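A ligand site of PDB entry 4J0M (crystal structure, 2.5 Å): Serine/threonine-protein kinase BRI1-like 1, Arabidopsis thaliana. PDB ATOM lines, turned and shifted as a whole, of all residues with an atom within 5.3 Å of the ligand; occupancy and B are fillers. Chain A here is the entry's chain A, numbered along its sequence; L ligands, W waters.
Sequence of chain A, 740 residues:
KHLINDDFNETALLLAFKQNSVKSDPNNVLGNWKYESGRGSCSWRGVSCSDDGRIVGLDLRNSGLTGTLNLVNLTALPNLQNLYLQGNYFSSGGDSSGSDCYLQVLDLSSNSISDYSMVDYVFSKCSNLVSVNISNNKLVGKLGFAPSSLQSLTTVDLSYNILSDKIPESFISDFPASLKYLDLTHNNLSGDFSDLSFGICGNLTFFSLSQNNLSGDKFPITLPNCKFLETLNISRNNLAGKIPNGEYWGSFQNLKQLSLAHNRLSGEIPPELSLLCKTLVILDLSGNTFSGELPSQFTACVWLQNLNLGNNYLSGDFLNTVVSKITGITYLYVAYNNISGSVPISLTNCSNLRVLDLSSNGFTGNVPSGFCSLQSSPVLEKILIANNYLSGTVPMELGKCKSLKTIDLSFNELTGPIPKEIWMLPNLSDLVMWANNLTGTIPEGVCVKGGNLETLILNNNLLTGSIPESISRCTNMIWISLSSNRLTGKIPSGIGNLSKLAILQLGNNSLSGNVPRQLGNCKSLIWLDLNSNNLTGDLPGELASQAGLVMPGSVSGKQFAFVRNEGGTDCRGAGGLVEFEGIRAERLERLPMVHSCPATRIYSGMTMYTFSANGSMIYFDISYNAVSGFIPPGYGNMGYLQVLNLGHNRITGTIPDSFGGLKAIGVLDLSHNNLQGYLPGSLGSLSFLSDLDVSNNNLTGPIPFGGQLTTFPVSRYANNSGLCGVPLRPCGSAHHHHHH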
ATOM      1  N   ILE A 503     -30.653 -18.893  -6.198  1.00  0.00           N
ATOM      2  CA  ILE A 503     -30.005 -20.159  -5.899  1.00  0.00           C
ATOM      3  C   ILE A 503     -30.879 -21.007  -4.989  1.00  0.00           C
ATOM      4  O   ILE A 503     -31.299 -20.558  -3.935  1.00  0.00           O
ATOM      5  CB  ILE A 503     -28.671 -19.909  -5.197  1.00  0.00           C
ATOM      6  CG1 ILE A 503     -27.764 -19.047  -6.088  1.00  0.00           C
ATOM      7  CG2 ILE A 503     -28.014 -21.213  -4.787  1.00  0.00           C
ATOM      8  CD1 ILE A 503     -26.546 -18.524  -5.393  1.00  0.00           C
ATOM      9  N   ILE A 526     -31.016 -19.201 -11.274  1.00  0.00           N
ATOM     10  CA  ILE A 526     -29.866 -19.628 -12.066  1.00  0.00           C
ATOM     11  C   ILE A 526     -29.167 -20.908 -11.597  1.00  0.00           C
ATOM     12  O   ILE A 526     -28.327 -21.470 -12.297  1.00  0.00           O
ATOM     13  CB  ILE A 526     -28.854 -18.470 -12.158  1.00  0.00           C
ATOM     14  CG1 ILE A 526     -28.259 -18.165 -10.781  1.00  0.00           C
ATOM     15  CG2 ILE A 526     -29.549 -17.220 -12.696  1.00  0.00           C
ATOM     16  CD1 ILE A 526     -27.186 -17.094 -10.802  1.00  0.00           C
ATOM     17  N   TRP A 527     -29.510 -21.353 -10.393  1.00  0.00           N
ATOM     18  CA  TRP A 527     -28.789 -22.459  -9.771  1.00  0.00           C
ATOM     19  C   TRP A 527     -29.753 -23.388  -9.036  1.00  0.00           C
ATOM     20  O   TRP A 527     -30.361 -22.982  -8.036  1.00  0.00           O
ATOM     21  CB  TRP A 527     -27.753 -21.918  -8.782  1.00  0.00           C
ATOM     22  CG  TRP A 527     -26.802 -22.918  -8.228  1.00  0.00           C
ATOM     23  CD1 TRP A 527     -27.088 -23.953  -7.355  1.00  0.00           C
ATOM     24  CD2 TRP A 527     -25.385 -22.991  -8.478  1.00  0.00           C
ATOM     25  NE1 TRP A 527     -25.928 -24.648  -7.057  1.00  0.00           N
ATOM     26  CE2 TRP A 527     -24.887 -24.085  -7.741  1.00  0.00           C
ATOM     27  CE3 TRP A 527     -24.493 -22.221  -9.245  1.00  0.00           C
ATOM     28  CZ2 TRP A 527     -23.532 -24.443  -7.749  1.00  0.00           C
ATOM     29  CZ3 TRP A 527     -23.161 -22.577  -9.263  1.00  0.00           C
ATOM     30  CH2 TRP A 527     -22.690 -23.675  -8.525  1.00  0.00           C
ATOM     31  N   PHE A 560     -18.860 -16.197  -1.543  1.00  0.00           N
ATOM     32  CA  PHE A 560     -19.093 -17.635  -1.718  1.00  0.00           C
ATOM     33  C   PHE A 560     -17.772 -18.362  -1.783  1.00  0.00           C
ATOM     34  O   PHE A 560     -16.705 -17.741  -1.928  1.00  0.00           O
ATOM     35  CB  PHE A 560     -19.819 -17.919  -3.023  1.00  0.00           C
ATOM     36  CG  PHE A 560     -18.910 -17.885  -4.216  1.00  0.00           C
ATOM     37  CD1 PHE A 560     -18.441 -19.060  -4.776  1.00  0.00           C
ATOM     38  CD2 PHE A 560     -18.470 -16.660  -4.738  1.00  0.00           C
ATOM     39  CE1 PHE A 560     -17.572 -19.030  -5.868  1.00  0.00           C
ATOM     40  CE2 PHE A 560     -17.595 -16.622  -5.830  1.00  0.00           C
ATOM     41  CZ  PHE A 560     -17.146 -17.808  -6.400  1.00  0.00           C
ATOM     42  N   PHE A 562     -16.478 -22.208  -3.731  1.00  0.00           N
ATOM     43  CA  PHE A 562     -16.854 -23.430  -4.432  1.00  0.00           C
ATOM     44  C   PHE A 562     -15.719 -24.445  -4.322  1.00  0.00           C
ATOM     45  O   PHE A 562     -14.622 -24.189  -4.816  1.00  0.00           O
ATOM     46  CB  PHE A 562     -17.171 -23.152  -5.895  1.00  0.00           C
ATOM     47  CG  PHE A 562     -17.741 -24.339  -6.632  1.00  0.00           C
ATOM     48  CD1 PHE A 562     -16.911 -25.164  -7.393  1.00  0.00           C
ATOM     49  CD2 PHE A 562     -19.097 -24.621  -6.582  1.00  0.00           C
ATOM     50  CE1 PHE A 562     -17.446 -26.264  -8.084  1.00  0.00           C
ATOM     51  CE2 PHE A 562     -19.626 -25.712  -7.263  1.00  0.00           C
ATOM     52  CZ  PHE A 562     -18.804 -26.531  -8.014  1.00  0.00           C
ATOM     53  N   ARG A 564     -13.914 -27.687  -5.372  1.00  0.00           N
ATOM     54  CA  ARG A 564     -13.790 -28.604  -6.484  1.00  0.00           C
ATOM     55  C   ARG A 564     -12.967 -29.826  -6.070  1.00  0.00           C
ATOM     56  O   ARG A 564     -11.916 -29.689  -5.438  1.00  0.00           O
ATOM     57  CB  ARG A 564     -13.113 -27.900  -7.655  1.00  0.00           C
ATOM     58  CG  ARG A 564     -13.096 -28.692  -8.949  1.00  0.00           C
ATOM     59  CD  ARG A 564     -12.401 -27.874 -10.014  1.00  0.00           C
ATOM     60  NE  ARG A 564     -12.353 -28.531 -11.313  1.00  0.00           N
ATOM     61  CZ  ARG A 564     -12.292 -27.878 -12.468  1.00  0.00           C
ATOM     62  NH1 ARG A 564     -12.294 -26.554 -12.474  1.00  0.00           N
ATOM     63  NH2 ARG A 564     -12.237 -28.543 -13.617  1.00  0.00           N
ATOM     64  N   LEU A 577     -20.827 -25.514  -3.750  1.00  0.00           N
ATOM     65  CA  LEU A 577     -21.011 -24.101  -3.484  1.00  0.00           C
ATOM     66  C   LEU A 577     -21.545 -23.798  -2.071  1.00  0.00           C
ATOM     67  O   LEU A 577     -22.586 -24.327  -1.659  1.00  0.00           O
ATOM     68  CB  LEU A 577     -21.932 -23.500  -4.565  1.00  0.00           C
ATOM     69  CG  LEU A 577     -22.428 -22.083  -4.362  1.00  0.00           C
ATOM     70  CD1 LEU A 577     -21.329 -21.116  -4.671  1.00  0.00           C
ATOM     71  CD2 LEU A 577     -23.637 -21.832  -5.244  1.00  0.00           C
ATOM     72  N   TYR A 603     -12.351 -22.202  -5.296  1.00  0.00           N
ATOM     73  CA  TYR A 603     -12.618 -20.841  -5.767  1.00  0.00           C
ATOM     74  C   TYR A 603     -13.314 -20.032  -4.678  1.00  0.00           C
ATOM     75  O   TYR A 603     -14.060 -20.572  -3.872  1.00  0.00           O
ATOM     76  CB  TYR A 603     -13.498 -20.871  -7.007  1.00  0.00           C
ATOM     77  CG  TYR A 603     -13.052 -21.814  -8.106  1.00  0.00           C
ATOM     78  CD1 TYR A 603     -13.230 -23.189  -7.974  1.00  0.00           C
ATOM     79  CD2 TYR A 603     -12.483 -21.340  -9.276  1.00  0.00           C
ATOM     80  CE1 TYR A 603     -12.845 -24.061  -8.974  1.00  0.00           C
ATOM     81  CE2 TYR A 603     -12.084 -22.210 -10.296  1.00  0.00           C
ATOM     82  CZ  TYR A 603     -12.273 -23.565 -10.135  1.00  0.00           C
ATOM     83  OH  TYR A 603     -11.893 -24.444 -11.124  1.00  0.00           O
ATOM     84  N   MET A 606     -16.495 -12.715  -4.568  1.00  0.00           N
ATOM     85  CA  MET A 606     -17.810 -12.122  -4.659  1.00  0.00           C
ATOM     86  C   MET A 606     -18.549 -12.813  -5.800  1.00  0.00           C
ATOM     87  O   MET A 606     -17.951 -13.092  -6.835  1.00  0.00           O
ATOM     88  CB  MET A 606     -17.665 -10.636  -4.984  1.00  0.00           C
ATOM     89  CG  MET A 606     -18.204  -9.705  -3.933  1.00  0.00           C
ATOM     90  SD  MET A 606     -17.631 -10.211  -2.317  1.00  0.00           S
ATOM     91  CE  MET A 606     -19.028  -9.701  -1.302  1.00  0.00           C
ATOM     92  N   THR A 607     -19.841 -13.071  -5.612  1.00  0.00           N
ATOM     93  CA  THR A 607     -20.625 -13.703  -6.673  1.00  0.00           C
ATOM     94  C   THR A 607     -20.880 -12.698  -7.783  1.00  0.00           C
ATOM     95  O   THR A 607     -21.279 -11.563  -7.523  1.00  0.00           O
ATOM     96  CB  THR A 607     -21.980 -14.266  -6.163  1.00  0.00           C
ATOM     97  OG1 THR A 607     -22.701 -13.229  -5.482  1.00  0.00           O
ATOM     98  CG2 THR A 607     -21.777 -15.436  -5.196  1.00  0.00           C
ATOM     99  N   MET A 608     -20.630 -13.113  -9.015  1.00  0.00           N
ATOM    100  CA  MET A 608     -20.973 -12.305 -10.176  1.00  0.00           C
ATOM    101  C   MET A 608     -21.618 -13.143 -11.284  1.00  0.00           C
ATOM    102  O   MET A 608     -21.182 -14.258 -11.586  1.00  0.00           O
ATOM    103  CB  MET A 608     -19.770 -11.505 -10.691  1.00  0.00           C
ATOM    104  CG  MET A 608     -19.046 -12.132 -11.857  1.00  0.00           C
ATOM    105  SD  MET A 608     -17.715 -11.074 -12.494  1.00  0.00           S
ATOM    106  CE  MET A 608     -16.872 -12.216 -13.595  1.00  0.00           C
ATOM    107  N   TYR A 609     -22.673 -12.596 -11.879  1.00  0.00           N
ATOM    108  CA  TYR A 609     -23.399 -13.268 -12.931  1.00  0.00           C
ATOM    109  C   TYR A 609     -22.529 -13.416 -14.186  1.00  0.00           C
ATOM    110  O   TYR A 609     -21.525 -12.729 -14.333  1.00  0.00           O
ATOM    111  CB  TYR A 609     -24.675 -12.494 -13.249  1.00  0.00           C
ATOM    112  CG  TYR A 609     -25.780 -12.743 -12.255  1.00  0.00           C
ATOM    113  CD1 TYR A 609     -26.926 -13.409 -12.646  1.00  0.00           C
ATOM    114  CD2 TYR A 609     -25.670 -12.316 -10.931  1.00  0.00           C
ATOM    115  CE1 TYR A 609     -27.947 -13.659 -11.744  1.00  0.00           C
ATOM    116  CE2 TYR A 609     -26.693 -12.552 -10.029  1.00  0.00           C
ATOM    117  CZ  TYR A 609     -27.838 -13.233 -10.450  1.00  0.00           C
ATOM    118  OH  TYR A 609     -28.865 -13.492  -9.577  1.00  0.00           O
ATOM    119  N   THR A 610     -22.891 -14.352 -15.047  1.00  0.00           N
ATOM    120  CA  THR A 610     -22.150 -14.582 -16.287  1.00  0.00           C
ATOM    121  C   THR A 610     -22.814 -13.908 -17.496  1.00  0.00           C
ATOM    122  O   THR A 610     -22.356 -14.072 -18.632  1.00  0.00           O
ATOM    123  CB  THR A 610     -21.936 -16.075 -16.540  1.00  0.00           C
ATOM    124  OG1 THR A 610     -23.210 -16.714 -16.680  1.00  0.00           O
ATOM    125  CG2 THR A 610     -21.192 -16.721 -15.374  1.00  0.00           C
ATOM    126  N   ILE A 618     -27.491 -21.262 -14.885  1.00  0.00           N
ATOM    127  CA  ILE A 618     -26.069 -21.645 -14.954  1.00  0.00           C
ATOM    128  C   ILE A 618     -25.827 -23.114 -14.579  1.00  0.00           C
ATOM    129  O   ILE A 618     -24.989 -23.803 -15.175  1.00  0.00           O
ATOM    130  CB  ILE A 618     -25.171 -20.758 -14.024  1.00  0.00           C
ATOM    131  CG1 ILE A 618     -25.463 -19.256 -14.179  1.00  0.00           C
ATOM    132  CG2 ILE A 618     -23.690 -21.057 -14.267  1.00  0.00           C
ATOM    133  CD1 ILE A 618     -26.012 -18.874 -15.521  1.00  0.00           C
ATOM    134  N   TYR A 619     -26.537 -23.584 -13.556  1.00  0.00           N
ATOM    135  CA  TYR A 619     -26.226 -24.845 -12.909  1.00  0.00           C
ATOM    136  C   TYR A 619     -27.486 -25.640 -12.603  1.00  0.00           C
ATOM    137  O   TYR A 619     -28.395 -25.142 -11.939  1.00  0.00           O
ATOM    138  CB  TYR A 619     -25.415 -24.560 -11.636  1.00  0.00           C
ATOM    139  CG  TYR A 619     -24.824 -25.767 -10.927  1.00  0.00           C
ATOM    140  CD1 TYR A 619     -25.595 -26.556 -10.092  1.00  0.00           C
ATOM    141  CD2 TYR A 619     -23.476 -26.065 -11.047  1.00  0.00           C
ATOM    142  CE1 TYR A 619     -25.059 -27.630  -9.416  1.00  0.00           C
ATOM    143  CE2 TYR A 619     -22.917 -27.142 -10.362  1.00  0.00           C
ATOM    144  CZ  TYR A 619     -23.720 -27.923  -9.557  1.00  0.00           C
ATOM    145  OH  TYR A 619     -23.183 -28.997  -8.881  1.00  0.00           O
ATOM    146  N   GLN A 642     -23.844 -23.993 -17.596  1.00  0.00           N
ATOM    147  CA  GLN A 642     -22.542 -24.641 -17.573  1.00  0.00           C
ATOM    148  C   GLN A 642     -22.508 -26.041 -16.975  1.00  0.00           C
ATOM    149  O   GLN A 642     -21.543 -26.773 -17.172  1.00  0.00           O
ATOM    150  CB  GLN A 642     -21.546 -23.770 -16.845  1.00  0.00           C
ATOM    151  CG  GLN A 642     -21.460 -22.389 -17.395  1.00  0.00           C
ATOM    152  CD  GLN A 642     -20.391 -21.606 -16.695  1.00  0.00           C
ATOM    153  OE1 GLN A 642     -19.247 -22.058 -16.615  1.00  0.00           O
ATOM    154  NE2 GLN A 642     -20.764 -20.450 -16.156  1.00  0.00           N
ATOM    155  N   VAL A 643     -23.565 -26.397 -16.248  1.00  0.00           N
ATOM    156  CA  VAL A 643     -23.625 -27.723 -15.671  1.00  0.00           C
ATOM    157  C   VAL A 643     -25.028 -28.285 -15.820  1.00  0.00           C
ATOM    158  O   VAL A 643     -26.018 -27.694 -15.378  1.00  0.00           O
ATOM    159  CB  VAL A 643     -23.193 -27.762 -14.188  1.00  0.00           C
ATOM    160  CG1 VAL A 643     -23.454 -29.168 -13.603  1.00  0.00           C
ATOM    161  CG2 VAL A 643     -21.723 -27.404 -14.053  1.00  0.00           C
ATOM    162  N   GLY A 666     -19.995 -26.818 -19.917  1.00  0.00           N
ATOM    163  CA  GLY A 666     -18.757 -27.505 -19.611  1.00  0.00           C
ATOM    164  C   GLY A 666     -18.942 -28.943 -19.117  1.00  0.00           C
ATOM    165  O   GLY A 666     -18.134 -29.816 -19.426  1.00  0.00           O
ATOM    166  N   VAL A 667     -20.025 -29.196 -18.394  1.00  0.00           N
ATOM    167  CA  VAL A 667     -20.253 -30.501 -17.773  1.00  0.00           C
ATOM    168  C   VAL A 667     -21.623 -31.050 -18.144  1.00  0.00           C
ATOM    169  O   VAL A 667     -22.654 -30.449 -17.831  1.00  0.00           O
ATOM    170  CB  VAL A 667     -20.102 -30.455 -16.237  1.00  0.00           C
ATOM    171  CG1 VAL A 667     -20.652 -31.734 -15.610  1.00  0.00           C
ATOM    172  CG2 VAL A 667     -18.661 -30.297 -15.874  1.00  0.00           C
ATOM    173  N   SER A 690     -16.090 -29.861 -21.442  1.00  0.00           N
ATOM    174  CA  SER A 690     -14.851 -30.440 -20.909  1.00  0.00           C
ATOM    175  C   SER A 690     -15.056 -31.729 -20.140  1.00  0.00           C
ATOM    176  O   SER A 690     -14.094 -32.448 -19.867  1.00  0.00           O
ATOM    177  CB  SER A 690     -14.163 -29.435 -20.009  1.00  0.00           C
ATOM    178  OG  SER A 690     -14.953 -29.224 -18.847  1.00  0.00           O
HETATM  179  C1  LIG L   1     -17.906 -25.920 -14.801  1.00  0.00           C
HETATM  180  C2  LIG L   1     -17.003 -26.602 -15.849  1.00  0.00           C
HETATM  181  O1  LIG L   1     -16.673 -25.715 -16.868  1.00  0.00           O
HETATM  182  C3  LIG L   1     -15.715 -27.217 -15.336  1.00  0.00           C
HETATM  183  O2  LIG L   1     -14.664 -26.390 -15.699  1.00  0.00           O
HETATM  184  C4  LIG L   1     -15.688 -27.476 -13.857  1.00  0.00           C
HETATM  185  C5  LIG L   1     -16.081 -26.244 -13.029  1.00  0.00           C
HETATM  186  C6  LIG L   1     -15.941 -26.567 -11.490  1.00  0.00           C
HETATM  187  O3  LIG L   1     -15.120 -27.651 -11.261  1.00  0.00           O
HETATM  188  C7  LIG L   1     -15.638 -24.284 -11.175  1.00  0.00           C
HETATM  189  O4  LIG L   1     -15.472 -25.563 -10.705  1.00  0.00           O
HETATM  190  C8  LIG L   1     -17.074 -23.886 -11.487  1.00  0.00           C
HETATM  191  C9  LIG L   1     -17.520 -24.114 -12.950  1.00  0.00           C
HETATM  192  C10 LIG L   1     -17.416 -25.627 -13.401  1.00  0.00           C
HETATM  193  C11 LIG L   1     -18.883 -23.487 -13.261  1.00  0.00           C
HETATM  194  C12 LIG L   1     -19.072 -22.045 -12.726  1.00  0.00           C
HETATM  195  C13 LIG L   1     -18.559 -21.754 -11.287  1.00  0.00           C
HETATM  196  C14 LIG L   1     -17.211 -22.387 -11.065  1.00  0.00           C
HETATM  197  C15 LIG L   1     -16.747 -21.955  -9.649  1.00  0.00           C
HETATM  198  C16 LIG L   1     -17.320 -20.526  -9.535  1.00  0.00           C
HETATM  199  C17 LIG L   1     -18.241 -20.369 -10.761  1.00  0.00           C
HETATM  200  C18 LIG L   1     -19.634 -22.455 -10.418  1.00  0.00           C
HETATM  201  C19 LIG L   1     -18.293 -26.375 -12.455  1.00  0.00           C
HETATM  202  C20 LIG L   1     -19.456 -19.505 -10.623  1.00  0.00           C
HETATM  203  C21 LIG L   1     -20.091 -19.319 -11.966  1.00  0.00           C
HETATM  204  C22 LIG L   1     -19.129 -18.143  -9.957  1.00  0.00           C
HETATM  205  O5  LIG L   1     -18.291 -17.486 -10.809  1.00  0.00           O
HETATM  206  C23 LIG L   1     -20.344 -17.279  -9.559  1.00  0.00           C
HETATM  207  O6  LIG L   1     -19.944 -16.181  -8.825  1.00  0.00           O
HETATM  208  C24 LIG L   1     -21.369 -18.137  -8.746  1.00  0.00           C
HETATM  209  C25 LIG L   1     -22.877 -17.721  -8.946  1.00  0.00           C
HETATM  210  C26 LIG L   1     -23.936 -18.663  -8.319  1.00  0.00           C
HETATM  211  C27 LIG L   1     -23.211 -17.183 -10.298  1.00  0.00           C
HETATM  212  C28 LIG L   1     -20.967 -18.292  -7.298  1.00  0.00           C
HETATM  213  O   HOH W   1     -18.409 -23.918 -18.792  1.00  0.00           O
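Water W1 lies within hydrogen-bond range of the side-chain amide oxygen of Gln 642, an oxygen (O1) of the ligand and the backbone NH of Gly 666.
An oxygen (O3) of the ligand is in hydrogen-bond range of the guanidinium group (NE) of Arg 564 (2.9 Å). An oxygen (O6) of the ligand is in hydrogen-bond range of the backbone NH (N) of Met 608, at 3.1 Å.
Residues that only touch the ligand: Thr 607 (3.4 Å), Phe 562 (3.4 Å), Tyr 603 (3.5 Å), Phe 560 (3.7 Å), Gln 642 (3.7 Å), Trp 527 (3.7 Å), Leu 577 (3.9 Å), Gly 666 (3.9 Å), Val 643 (3.9 Å) and Ile 503 (3.9 Å). Within 4 Å of the ligand: Ile 503, Trp 527, Phe 560, Phe 562, Arg 564, Leu 577, Tyr 603, Thr 607, Met 608, Gln 642, Val 643 and Gly 666.
The guanidinium group of Arg 564 lies within hydrogen-bond range of the side-chain hydroxyl of Tyr 603, at 2.5 Å. N of Phe 562 lies within hydrogen-bond range of O of Tyr 603 (2.9 Å). O of Gln 642 lies within hydrogen-bond range of N of Gly 666 (3.2 Å). O of Gln 642 sits at hydrogen-bond distance from N of Val 667 (3.1 Å). The backbone NH of Gln 642 lies within hydrogen-bond range of the backbone carbonyl oxygen of Ile 618, at 2.7 Å. The backbone carbonyl oxygen of Gly 666 lies within hydrogen-bond range of the backbone NH of Ser 690 (2.9 Å). N of Val 643 sits at hydrogen-bond distance from O of Ile 618.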
